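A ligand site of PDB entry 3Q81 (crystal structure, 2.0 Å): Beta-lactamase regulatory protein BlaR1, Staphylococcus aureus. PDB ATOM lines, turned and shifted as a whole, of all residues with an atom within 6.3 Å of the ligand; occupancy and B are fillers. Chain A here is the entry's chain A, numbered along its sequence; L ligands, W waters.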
ATOM      1  N   PRO A  56      16.301 -19.528  29.159  1.00  0.00           N
ATOM      2  CA  PRO A  56      16.774 -20.845  29.470  1.00  0.00           C
ATOM      3  C   PRO A  56      16.085 -21.939  28.629  1.00  0.00           C
ATOM      4  O   PRO A  56      16.641 -23.032  28.521  1.00  0.00           O
ATOM      5  CB  PRO A  56      16.382 -21.026  30.919  1.00  0.00           C
ATOM      6  CG  PRO A  56      15.141 -20.085  31.085  1.00  0.00           C
ATOM      7  CD  PRO A  56      15.568 -18.923  30.301  1.00  0.00           C
ATOM      8  N   ASN A  57      14.921 -21.624  28.034  1.00  0.00           N
ATOM      9  CA  ASN A  57      14.080 -22.606  27.329  1.00  0.00           C
ATOM     10  C   ASN A  57      13.918 -23.889  28.159  1.00  0.00           C
ATOM     11  O   ASN A  57      13.627 -23.787  29.353  1.00  0.00           O
ATOM     12  CB  ASN A  57      14.541 -22.801  25.870  1.00  0.00           C
ATOM     13  CG  ASN A  57      14.371 -21.544  25.053  1.00  0.00           C
ATOM     14  OD1 ASN A  57      13.270 -20.983  24.971  1.00  0.00           O
ATOM     15  ND2 ASN A  57      15.452 -21.051  24.465  1.00  0.00           N
ATOM     16  N   SER A  58      14.219 -25.059  27.597  1.00  0.00           N
ATOM     17  CA  SER A  58      13.892 -26.354  28.253  1.00  0.00           C
ATOM     18  C   SER A  58      14.807 -26.669  29.417  1.00  0.00           C
ATOM     19  O   SER A  58      14.470 -27.546  30.220  1.00  0.00           O
ATOM     20  CB  SER A  58      13.879 -27.503  27.238  1.00  0.00           C
ATOM     21  OG  SER A  58      12.860 -27.191  26.292  1.00  0.00           O
ATOM     22  N   THR A  59      15.917 -25.945  29.576  1.00  0.00           N
ATOM     23  CA  THR A  59      16.767 -26.167  30.764  1.00  0.00           C
ATOM     24  C   THR A  59      16.029 -25.765  32.041  1.00  0.00           C
ATOM     25  O   THR A  59      16.309 -26.320  33.075  1.00  0.00           O
ATOM     26  CB  THR A  59      18.129 -25.470  30.702  1.00  0.00           C
ATOM     27  OG1 THR A  59      17.949 -24.052  30.705  1.00  0.00           O
ATOM     28  CG2 THR A  59      18.888 -25.918  29.444  1.00  0.00           C
ATOM     29  N   LYS A  61      13.117 -26.561  32.792  1.00  0.00           N
ATOM     30  CA  LYS A  61      12.390 -27.750  33.245  1.00  0.00           C
ATOM     31  C   LYS A  61      13.063 -28.483  34.424  1.00  0.00           C
ATOM     32  O   LYS A  61      12.371 -29.166  35.163  1.00  0.00           O
ATOM     33  CB  LYS A  61      12.164 -28.730  32.110  1.00  0.00           C
ATOM     34  CG  LYS A  61      11.189 -28.200  31.053  1.00  0.00           C
ATOM     35  CD  LYS A  61      11.359 -28.922  29.764  1.00  0.00           C
ATOM     36  CE  LYS A  61      10.206 -28.465  28.844  1.00  0.00           C
ATOM     37  NZ  LYS A  61      10.243 -29.285  27.627  1.00  0.00           N
ATOM     38  N   PHE A  90       5.436 -34.767  17.457  1.00  0.00           N
ATOM     39  CA  PHE A  90       6.335 -35.860  17.887  1.00  0.00           C
ATOM     40  C   PHE A  90       5.543 -36.847  18.725  1.00  0.00           C
ATOM     41  O   PHE A  90       4.963 -36.472  19.749  1.00  0.00           O
ATOM     42  CB  PHE A  90       7.489 -35.325  18.725  1.00  0.00           C
ATOM     43  CG  PHE A  90       7.995 -33.990  18.278  1.00  0.00           C
ATOM     44  CD1 PHE A  90       7.801 -32.864  19.085  1.00  0.00           C
ATOM     45  CD2 PHE A  90       8.673 -33.836  17.067  1.00  0.00           C
ATOM     46  CE1 PHE A  90       8.289 -31.594  18.699  1.00  0.00           C
ATOM     47  CE2 PHE A  90       9.154 -32.589  16.658  1.00  0.00           C
ATOM     48  CZ  PHE A  90       8.958 -31.456  17.481  1.00  0.00           C
ATOM     49  N   ASP A  91       5.535 -38.122  18.301  1.00  0.00           N
ATOM     50  CA  ASP A  91       4.717 -39.165  18.955  1.00  0.00           C
ATOM     51  C   ASP A  91       5.077 -39.458  20.405  1.00  0.00           C
ATOM     52  O   ASP A  91       4.202 -39.974  21.133  1.00  0.00           O
ATOM     53  CB  ASP A  91       4.715 -40.476  18.162  1.00  0.00           C
ATOM     54  CG  ASP A  91       3.798 -40.446  16.966  1.00  0.00           C
ATOM     55  OD1 ASP A  91       4.110 -41.206  16.034  1.00  0.00           O
ATOM     56  OD2 ASP A  91       2.774 -39.703  16.930  1.00  0.00           O
ATOM     57  N   ALA A  92       6.295 -39.075  20.828  1.00  0.00           N
ATOM     58  CA  ALA A  92       6.779 -39.237  22.202  1.00  0.00           C
ATOM     59  C   ALA A  92       6.008 -38.333  23.163  1.00  0.00           C
ATOM     60  O   ALA A  92       5.948 -38.599  24.361  1.00  0.00           O
ATOM     61  CB  ALA A  92       8.284 -38.939  22.290  1.00  0.00           C
ATOM     62  N   TRP A  93       5.415 -37.271  22.627  1.00  0.00           N
ATOM     63  CA  TRP A  93       4.555 -36.356  23.368  1.00  0.00           C
ATOM     64  C   TRP A  93       3.100 -36.824  23.402  1.00  0.00           C
ATOM     65  O   TRP A  93       2.360 -36.453  24.313  1.00  0.00           O
ATOM     66  CB  TRP A  93       4.554 -34.980  22.700  1.00  0.00           C
ATOM     67  CG  TRP A  93       5.820 -34.188  22.792  1.00  0.00           C
ATOM     68  CD1 TRP A  93       7.104 -34.667  22.889  1.00  0.00           C
ATOM     69  CD2 TRP A  93       5.923 -32.778  22.726  1.00  0.00           C
ATOM     70  NE1 TRP A  93       7.992 -33.629  22.947  1.00  0.00           N
ATOM     71  CE2 TRP A  93       7.301 -32.449  22.837  1.00  0.00           C
ATOM     72  CE3 TRP A  93       4.995 -31.740  22.589  1.00  0.00           C
ATOM     73  CZ2 TRP A  93       7.751 -31.134  22.818  1.00  0.00           C
ATOM     74  CZ3 TRP A  93       5.461 -30.431  22.588  1.00  0.00           C
ATOM     75  CH2 TRP A  93       6.813 -30.141  22.682  1.00  0.00           C
ATOM     76  N   GLN A 104      13.289 -36.657  29.494  1.00  0.00           N
ATOM     77  CA  GLN A 104      14.081 -37.266  28.421  1.00  0.00           C
ATOM     78  C   GLN A 104      13.633 -36.784  27.035  1.00  0.00           C
ATOM     79  O   GLN A 104      14.449 -36.482  26.161  1.00  0.00           O
ATOM     80  CB  GLN A 104      13.919 -38.798  28.479  1.00  0.00           C
ATOM     81  CG  GLN A 104      14.793 -39.558  27.497  1.00  0.00           C
ATOM     82  CD  GLN A 104      14.531 -41.028  27.465  1.00  0.00           C
ATOM     83  OE1 GLN A 104      14.227 -41.654  28.482  1.00  0.00           O
ATOM     84  NE2 GLN A 104      14.603 -41.601  26.290  1.00  0.00           N
ATOM     85  N   ASN A 105      12.330 -36.725  26.839  1.00  0.00           N
ATOM     86  CA  ASN A 105      11.819 -36.327  25.567  1.00  0.00           C
ATOM     87  C   ASN A 105      11.345 -34.868  25.544  1.00  0.00           C
ATOM     88  O   ASN A 105      10.701 -34.480  24.580  1.00  0.00           O
ATOM     89  CB  ASN A 105      10.702 -37.285  25.119  1.00  0.00           C
ATOM     90  CG  ASN A 105      11.191 -38.741  24.994  1.00  0.00           C
ATOM     91  OD1 ASN A 105      12.149 -39.007  24.286  1.00  0.00           O
ATOM     92  ND2 ASN A 105      10.494 -39.674  25.652  1.00  0.00           N
ATOM     93  N   SER A 106      11.673 -34.099  26.589  1.00  0.00           N
ATOM     94  CA  SER A 106      11.420 -32.640  26.658  1.00  0.00           C
ATOM     95  C   SER A 106       9.972 -32.294  26.257  1.00  0.00           C
ATOM     96  O   SER A 106       9.733 -31.561  25.273  1.00  0.00           O
ATOM     97  CB  SER A 106      12.424 -31.865  25.806  1.00  0.00           C
ATOM     98  OG  SER A 106      12.678 -30.601  26.402  1.00  0.00           O
ATOM     99  N   VAL A 107       9.024 -32.840  27.013  1.00  0.00           N
ATOM    100  CA  VAL A 107       7.626 -32.805  26.627  1.00  0.00           C
ATOM    101  C   VAL A 107       7.052 -31.566  27.276  1.00  0.00           C
ATOM    102  O   VAL A 107       6.797 -31.555  28.486  1.00  0.00           O
ATOM    103  CB  VAL A 107       6.845 -34.085  27.109  1.00  0.00           C
ATOM    104  CG1 VAL A 107       5.367 -33.957  26.737  1.00  0.00           C
ATOM    105  CG2 VAL A 107       7.393 -35.385  26.466  1.00  0.00           C
ATOM    106  N   ASN A 108       6.855 -30.511  26.474  1.00  0.00           N
ATOM    107  CA  ASN A 108       6.457 -29.192  27.002  1.00  0.00           C
ATOM    108  C   ASN A 108       5.202 -29.219  27.831  1.00  0.00           C
ATOM    109  O   ASN A 108       5.147 -28.574  28.871  1.00  0.00           O
ATOM    110  CB  ASN A 108       6.219 -28.191  25.883  1.00  0.00           C
ATOM    111  CG  ASN A 108       7.500 -27.747  25.207  1.00  0.00           C
ATOM    112  OD1 ASN A 108       8.624 -28.074  25.620  1.00  0.00           O
ATOM    113  ND2 ASN A 108       7.317 -27.001  24.142  1.00  0.00           N
ATOM    114  N   TRP A 144       9.618 -18.904  30.582  1.00  0.00           N
ATOM    115  CA  TRP A 144      10.918 -19.477  30.346  1.00  0.00           C
ATOM    116  C   TRP A 144      11.172 -19.795  28.889  1.00  0.00           C
ATOM    117  O   TRP A 144      12.254 -20.305  28.582  1.00  0.00           O
ATOM    118  CB  TRP A 144      11.117 -20.758  31.147  1.00  0.00           C
ATOM    119  CG  TRP A 144      10.197 -21.901  30.734  1.00  0.00           C
ATOM    120  CD1 TRP A 144      10.488 -22.934  29.858  1.00  0.00           C
ATOM    121  CD2 TRP A 144       8.858 -22.127  31.180  1.00  0.00           C
ATOM    122  NE1 TRP A 144       9.405 -23.769  29.751  1.00  0.00           N
ATOM    123  CE2 TRP A 144       8.392 -23.300  30.559  1.00  0.00           C
ATOM    124  CE3 TRP A 144       8.018 -21.453  32.078  1.00  0.00           C
ATOM    125  CZ2 TRP A 144       7.107 -23.796  30.769  1.00  0.00           C
ATOM    126  CZ3 TRP A 144       6.747 -21.945  32.288  1.00  0.00           C
ATOM    127  CH2 TRP A 144       6.298 -23.100  31.629  1.00  0.00           C
ATOM    128  N   MET A 145      10.210 -19.526  27.991  1.00  0.00           N
ATOM    129  CA  MET A 145      10.396 -19.837  26.559  1.00  0.00           C
ATOM    130  C   MET A 145      10.471 -18.583  25.716  1.00  0.00           C
ATOM    131  O   MET A 145       9.439 -18.002  25.396  1.00  0.00           O
ATOM    132  CB  MET A 145       9.266 -20.726  26.024  1.00  0.00           C
ATOM    133  CG  MET A 145       9.072 -22.048  26.726  1.00  0.00           C
ATOM    134  SD  MET A 145       7.624 -23.031  26.168  1.00  0.00           S
ATOM    135  CE  MET A 145       7.809 -22.965  24.374  1.00  0.00           C
ATOM    136  N   LYS A 195      20.523 -31.674  30.590  1.00  0.00           N
ATOM    137  CA  LYS A 195      19.265 -31.267  29.943  1.00  0.00           C
ATOM    138  C   LYS A 195      19.556 -30.256  28.830  1.00  0.00           C
ATOM    139  O   LYS A 195      20.264 -29.283  29.040  1.00  0.00           O
ATOM    140  CB  LYS A 195      18.278 -30.696  30.946  1.00  0.00           C
ATOM    141  CG  LYS A 195      16.907 -30.209  30.334  1.00  0.00           C
ATOM    142  CD  LYS A 195      16.009 -31.375  29.883  1.00  0.00           C
ATOM    143  CE  LYS A 195      14.776 -30.854  29.075  1.00  0.00           C
ATOM    144  NZ  LYS A 195      15.198 -30.919  27.632  1.00  0.00           N
ATOM    145  N   THR A 196      19.046 -30.545  27.648  1.00  0.00           N
ATOM    146  CA  THR A 196      19.196 -29.652  26.519  1.00  0.00           C
ATOM    147  C   THR A 196      18.107 -28.554  26.561  1.00  0.00           C
ATOM    148  O   THR A 196      17.059 -28.696  27.245  1.00  0.00           O
ATOM    149  CB  THR A 196      19.061 -30.416  25.209  1.00  0.00           C
ATOM    150  OG1 THR A 196      17.835 -31.171  25.210  1.00  0.00           O
ATOM    151  CG2 THR A 196      20.249 -31.376  25.019  1.00  0.00           C
ATOM    152  N   GLY A 197      18.368 -27.499  25.804  1.00  0.00           N
ATOM    153  CA  GLY A 197      17.397 -26.466  25.592  1.00  0.00           C
ATOM    154  C   GLY A 197      17.657 -25.881  24.232  1.00  0.00           C
ATOM    155  O   GLY A 197      18.828 -25.664  23.875  1.00  0.00           O
ATOM    156  N   THR A 198      16.586 -25.671  23.457  1.00  0.00           N
ATOM    157  CA  THR A 198      16.688 -25.029  22.161  1.00  0.00           C
ATOM    158  C   THR A 198      15.595 -23.987  22.017  1.00  0.00           C
ATOM    159  O   THR A 198      14.422 -24.290  22.229  1.00  0.00           O
ATOM    160  CB  THR A 198      16.512 -26.026  20.965  1.00  0.00           C
ATOM    161  OG1 THR A 198      17.212 -27.238  21.228  1.00  0.00           O
ATOM    162  CG2 THR A 198      17.082 -25.417  19.719  1.00  0.00           C
ATOM    163  N   GLY A 199      15.966 -22.771  21.665  1.00  0.00           N
ATOM    164  CA  GLY A 199      15.015 -21.751  21.307  1.00  0.00           C
ATOM    165  C   GLY A 199      14.940 -21.590  19.815  1.00  0.00           C
ATOM    166  O   GLY A 199      15.976 -21.506  19.139  1.00  0.00           O
ATOM    167  N   TRP A 209      21.396 -24.886  24.502  1.00  0.00           N
ATOM    168  CA  TRP A 209      21.950 -25.063  25.836  1.00  0.00           C
ATOM    169  C   TRP A 209      22.161 -26.535  26.039  1.00  0.00           C
ATOM    170  O   TRP A 209      21.494 -27.365  25.397  1.00  0.00           O
ATOM    171  CB  TRP A 209      20.919 -24.712  26.893  1.00  0.00           C
ATOM    172  CG  TRP A 209      20.546 -23.275  27.161  1.00  0.00           C
ATOM    173  CD1 TRP A 209      19.372 -22.665  26.831  1.00  0.00           C
ATOM    174  CD2 TRP A 209      21.303 -22.307  27.905  1.00  0.00           C
ATOM    175  NE1 TRP A 209      19.379 -21.363  27.279  1.00  0.00           N
ATOM    176  CE2 TRP A 209      20.535 -21.122  27.955  1.00  0.00           C
ATOM    177  CE3 TRP A 209      22.563 -22.333  28.531  1.00  0.00           C
ATOM    178  CZ2 TRP A 209      20.983 -19.962  28.605  1.00  0.00           C
ATOM    179  CZ3 TRP A 209      22.997 -21.178  29.181  1.00  0.00           C
ATOM    180  CH2 TRP A 209      22.206 -20.013  29.224  1.00  0.00           C
ATOM    181  N   SER A 233      21.791 -25.121  18.424  1.00  0.00           N
ATOM    182  CA  SER A 233      20.804 -26.044  18.949  1.00  0.00           C
ATOM    183  C   SER A 233      21.250 -26.711  20.275  1.00  0.00           C
ATOM    184  O   SER A 233      22.449 -26.748  20.599  1.00  0.00           O
ATOM    185  CB  SER A 233      20.436 -27.116  17.913  1.00  0.00           C
ATOM    186  OG  SER A 233      21.490 -28.073  17.732  1.00  0.00           O
ATOM    187  N   GLY A 234      20.277 -27.247  20.984  1.00  0.00           N
ATOM    188  CA  GLY A 234      20.512 -28.048  22.194  1.00  0.00           C
ATOM    189  C   GLY A 234      21.351 -29.291  21.910  1.00  0.00           C
ATOM    190  O   GLY A 234      22.260 -29.599  22.683  1.00  0.00           O
ATOM    191  N   LYS A 235      21.078 -29.944  20.779  1.00  0.00           N
ATOM    192  CA  LYS A 235      21.813 -31.135  20.346  1.00  0.00           C
ATOM    193  C   LYS A 235      23.289 -30.805  20.103  1.00  0.00           C
ATOM    194  O   LYS A 235      24.187 -31.532  20.583  1.00  0.00           O
ATOM    195  CB  LYS A 235      21.182 -31.727  19.084  1.00  0.00           C
ATOM    196  CG  LYS A 235      21.831 -33.022  18.610  1.00  0.00           C
ATOM    197  CD  LYS A 235      21.149 -33.644  17.375  1.00  0.00           C
ATOM    198  CE  LYS A 235      22.178 -34.479  16.615  1.00  0.00           C
ATOM    199  NZ  LYS A 235      21.553 -35.588  15.836  1.00  0.00           N
HETATM  200  C1  LIG L   1      13.162 -26.722  24.969  1.00  0.00           C
HETATM  201  C2  LIG L   1      13.033 -29.879  22.437  1.00  0.00           C
HETATM  202  C3  LIG L   1      12.200 -26.836  23.796  1.00  0.00           C
HETATM  203  C4  LIG L   1      11.698 -28.290  23.570  1.00  0.00           C
HETATM  204  C5  LIG L   1      13.758 -29.391  23.394  1.00  0.00           C
HETATM  205  O1  LIG L   1      14.248 -26.203  24.789  1.00  0.00           O
HETATM  206  C6  LIG L   1      11.212 -25.658  23.887  1.00  0.00           C
HETATM  207  O2  LIG L   1      10.991 -25.057  25.155  1.00  0.00           O
HETATM  208  C7  LIG L   1       9.922 -25.895  23.131  1.00  0.00           C
HETATM  209  N1  LIG L   1      12.867 -28.911  24.145  1.00  0.00           N
HETATM  210  C8  LIG L   1      15.222 -29.378  23.715  1.00  0.00           C
HETATM  211  O3  LIG L   1      15.516 -29.859  24.819  1.00  0.00           O
HETATM  212  O4  LIG L   1      16.171 -28.907  22.988  1.00  0.00           O
HETATM  213  S1  LIG L   1      13.407 -31.383  21.852  1.00  0.00           S
HETATM  214  C9  LIG L   1      12.252 -32.712  21.900  1.00  0.00           C
HETATM  215  C10 LIG L   1      11.867 -33.140  20.481  1.00  0.00           C
HETATM  216  N2  LIG L   1      10.913 -34.254  20.463  1.00  0.00           N
HETATM  217  C11 LIG L   1      11.148 -35.358  21.178  1.00  0.00           C
HETATM  218  N3  LIG L   1      10.326 -36.324  21.147  1.00  0.00           N
HETATM  219  C12 LIG L   1      11.854 -28.963  22.185  1.00  0.00           C
HETATM  220  O   HOH W   1      11.893 -24.692  20.916  1.00  0.00           O
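Asn 57 touches the ligand (CB to O1, 3.6 Å). CG of Phe 90 touches N2 of the ligand, 3.7 Å away. Ala 92 touches the ligand. Trp 93 touches the ligand. Asn 105 touches the ligand (O to C11, 3.5 Å). ND2 of Asn 108 touches C7 of the ligand (3.0 Å). Met 145 touches the ligand. Gly 197 touches the ligand. Of the 25 residues printed, 13 come within 4 Å of the ligand. The nearest printed residue that does not touch the ligand is Lys 61 (4.4 Å).
The side-chain amino group (NZ) of Lys 61 is in hydrogen-bond range of the side-chain amide oxygen (OD1) of Asn 108, at 2.8 Å. OG of Ser 58 sits at hydrogen-bond distance from OG of Ser 106 (3.4 Å). The side-chain hydroxyl (OG) of Ser 106 sits at hydrogen-bond distance from the side-chain amino group (NZ) of Lys 195 (2.8 Å). The backbone carbonyl oxygen (O) of Asn 105 lies within hydrogen-bond range of the indole nitrogen (NE1) of Trp 93 (3.3 Å). The side-chain amide nitrogen of Asn 57 lies close to the backbone NH of Gly 199, 3.3 Å away. The backbone carbonyl oxygen (O) of Trp 144 lies within hydrogen-bond range of the backbone NH (N) of Asn 57 (3.0 Å). The side-chain amino group (NZ) of Lys 61 is in hydrogen-bond range of the side-chain hydroxyl (OG) of Ser 106 (3.0 Å). The side-chain hydroxyl (OG1) of Thr 198 is in hydrogen-bond range of the backbone NH (N) of Gly 234, 3.1 Å away.
The backbone NH (N) of Thr 198 is in hydrogen-bond range of an oxygen (O1) of the ligand (2.7 Å). The side-chain amino group of Lys 195 lies within salt-bridge range of an oxygen (O3) of the ligand. OG of Ser 106 is in hydrogen-bond range of N1 of the ligand. An oxygen (O1) of the ligand sits close to the backbone NH (N) of Ser 58, 3.0 Å away. A carbon (C1) of the ligand is bonded to the side-chain hydroxyl (OG) of Ser 58. OG1 of Thr 196 lies within hydrogen-bond range of O3 of the ligand (2.7 Å). The side-chain hydroxyl (OG1) of Thr 198 lies within hydrogen-bond range of an oxygen (O4) of the ligand, 2.6 Å away.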
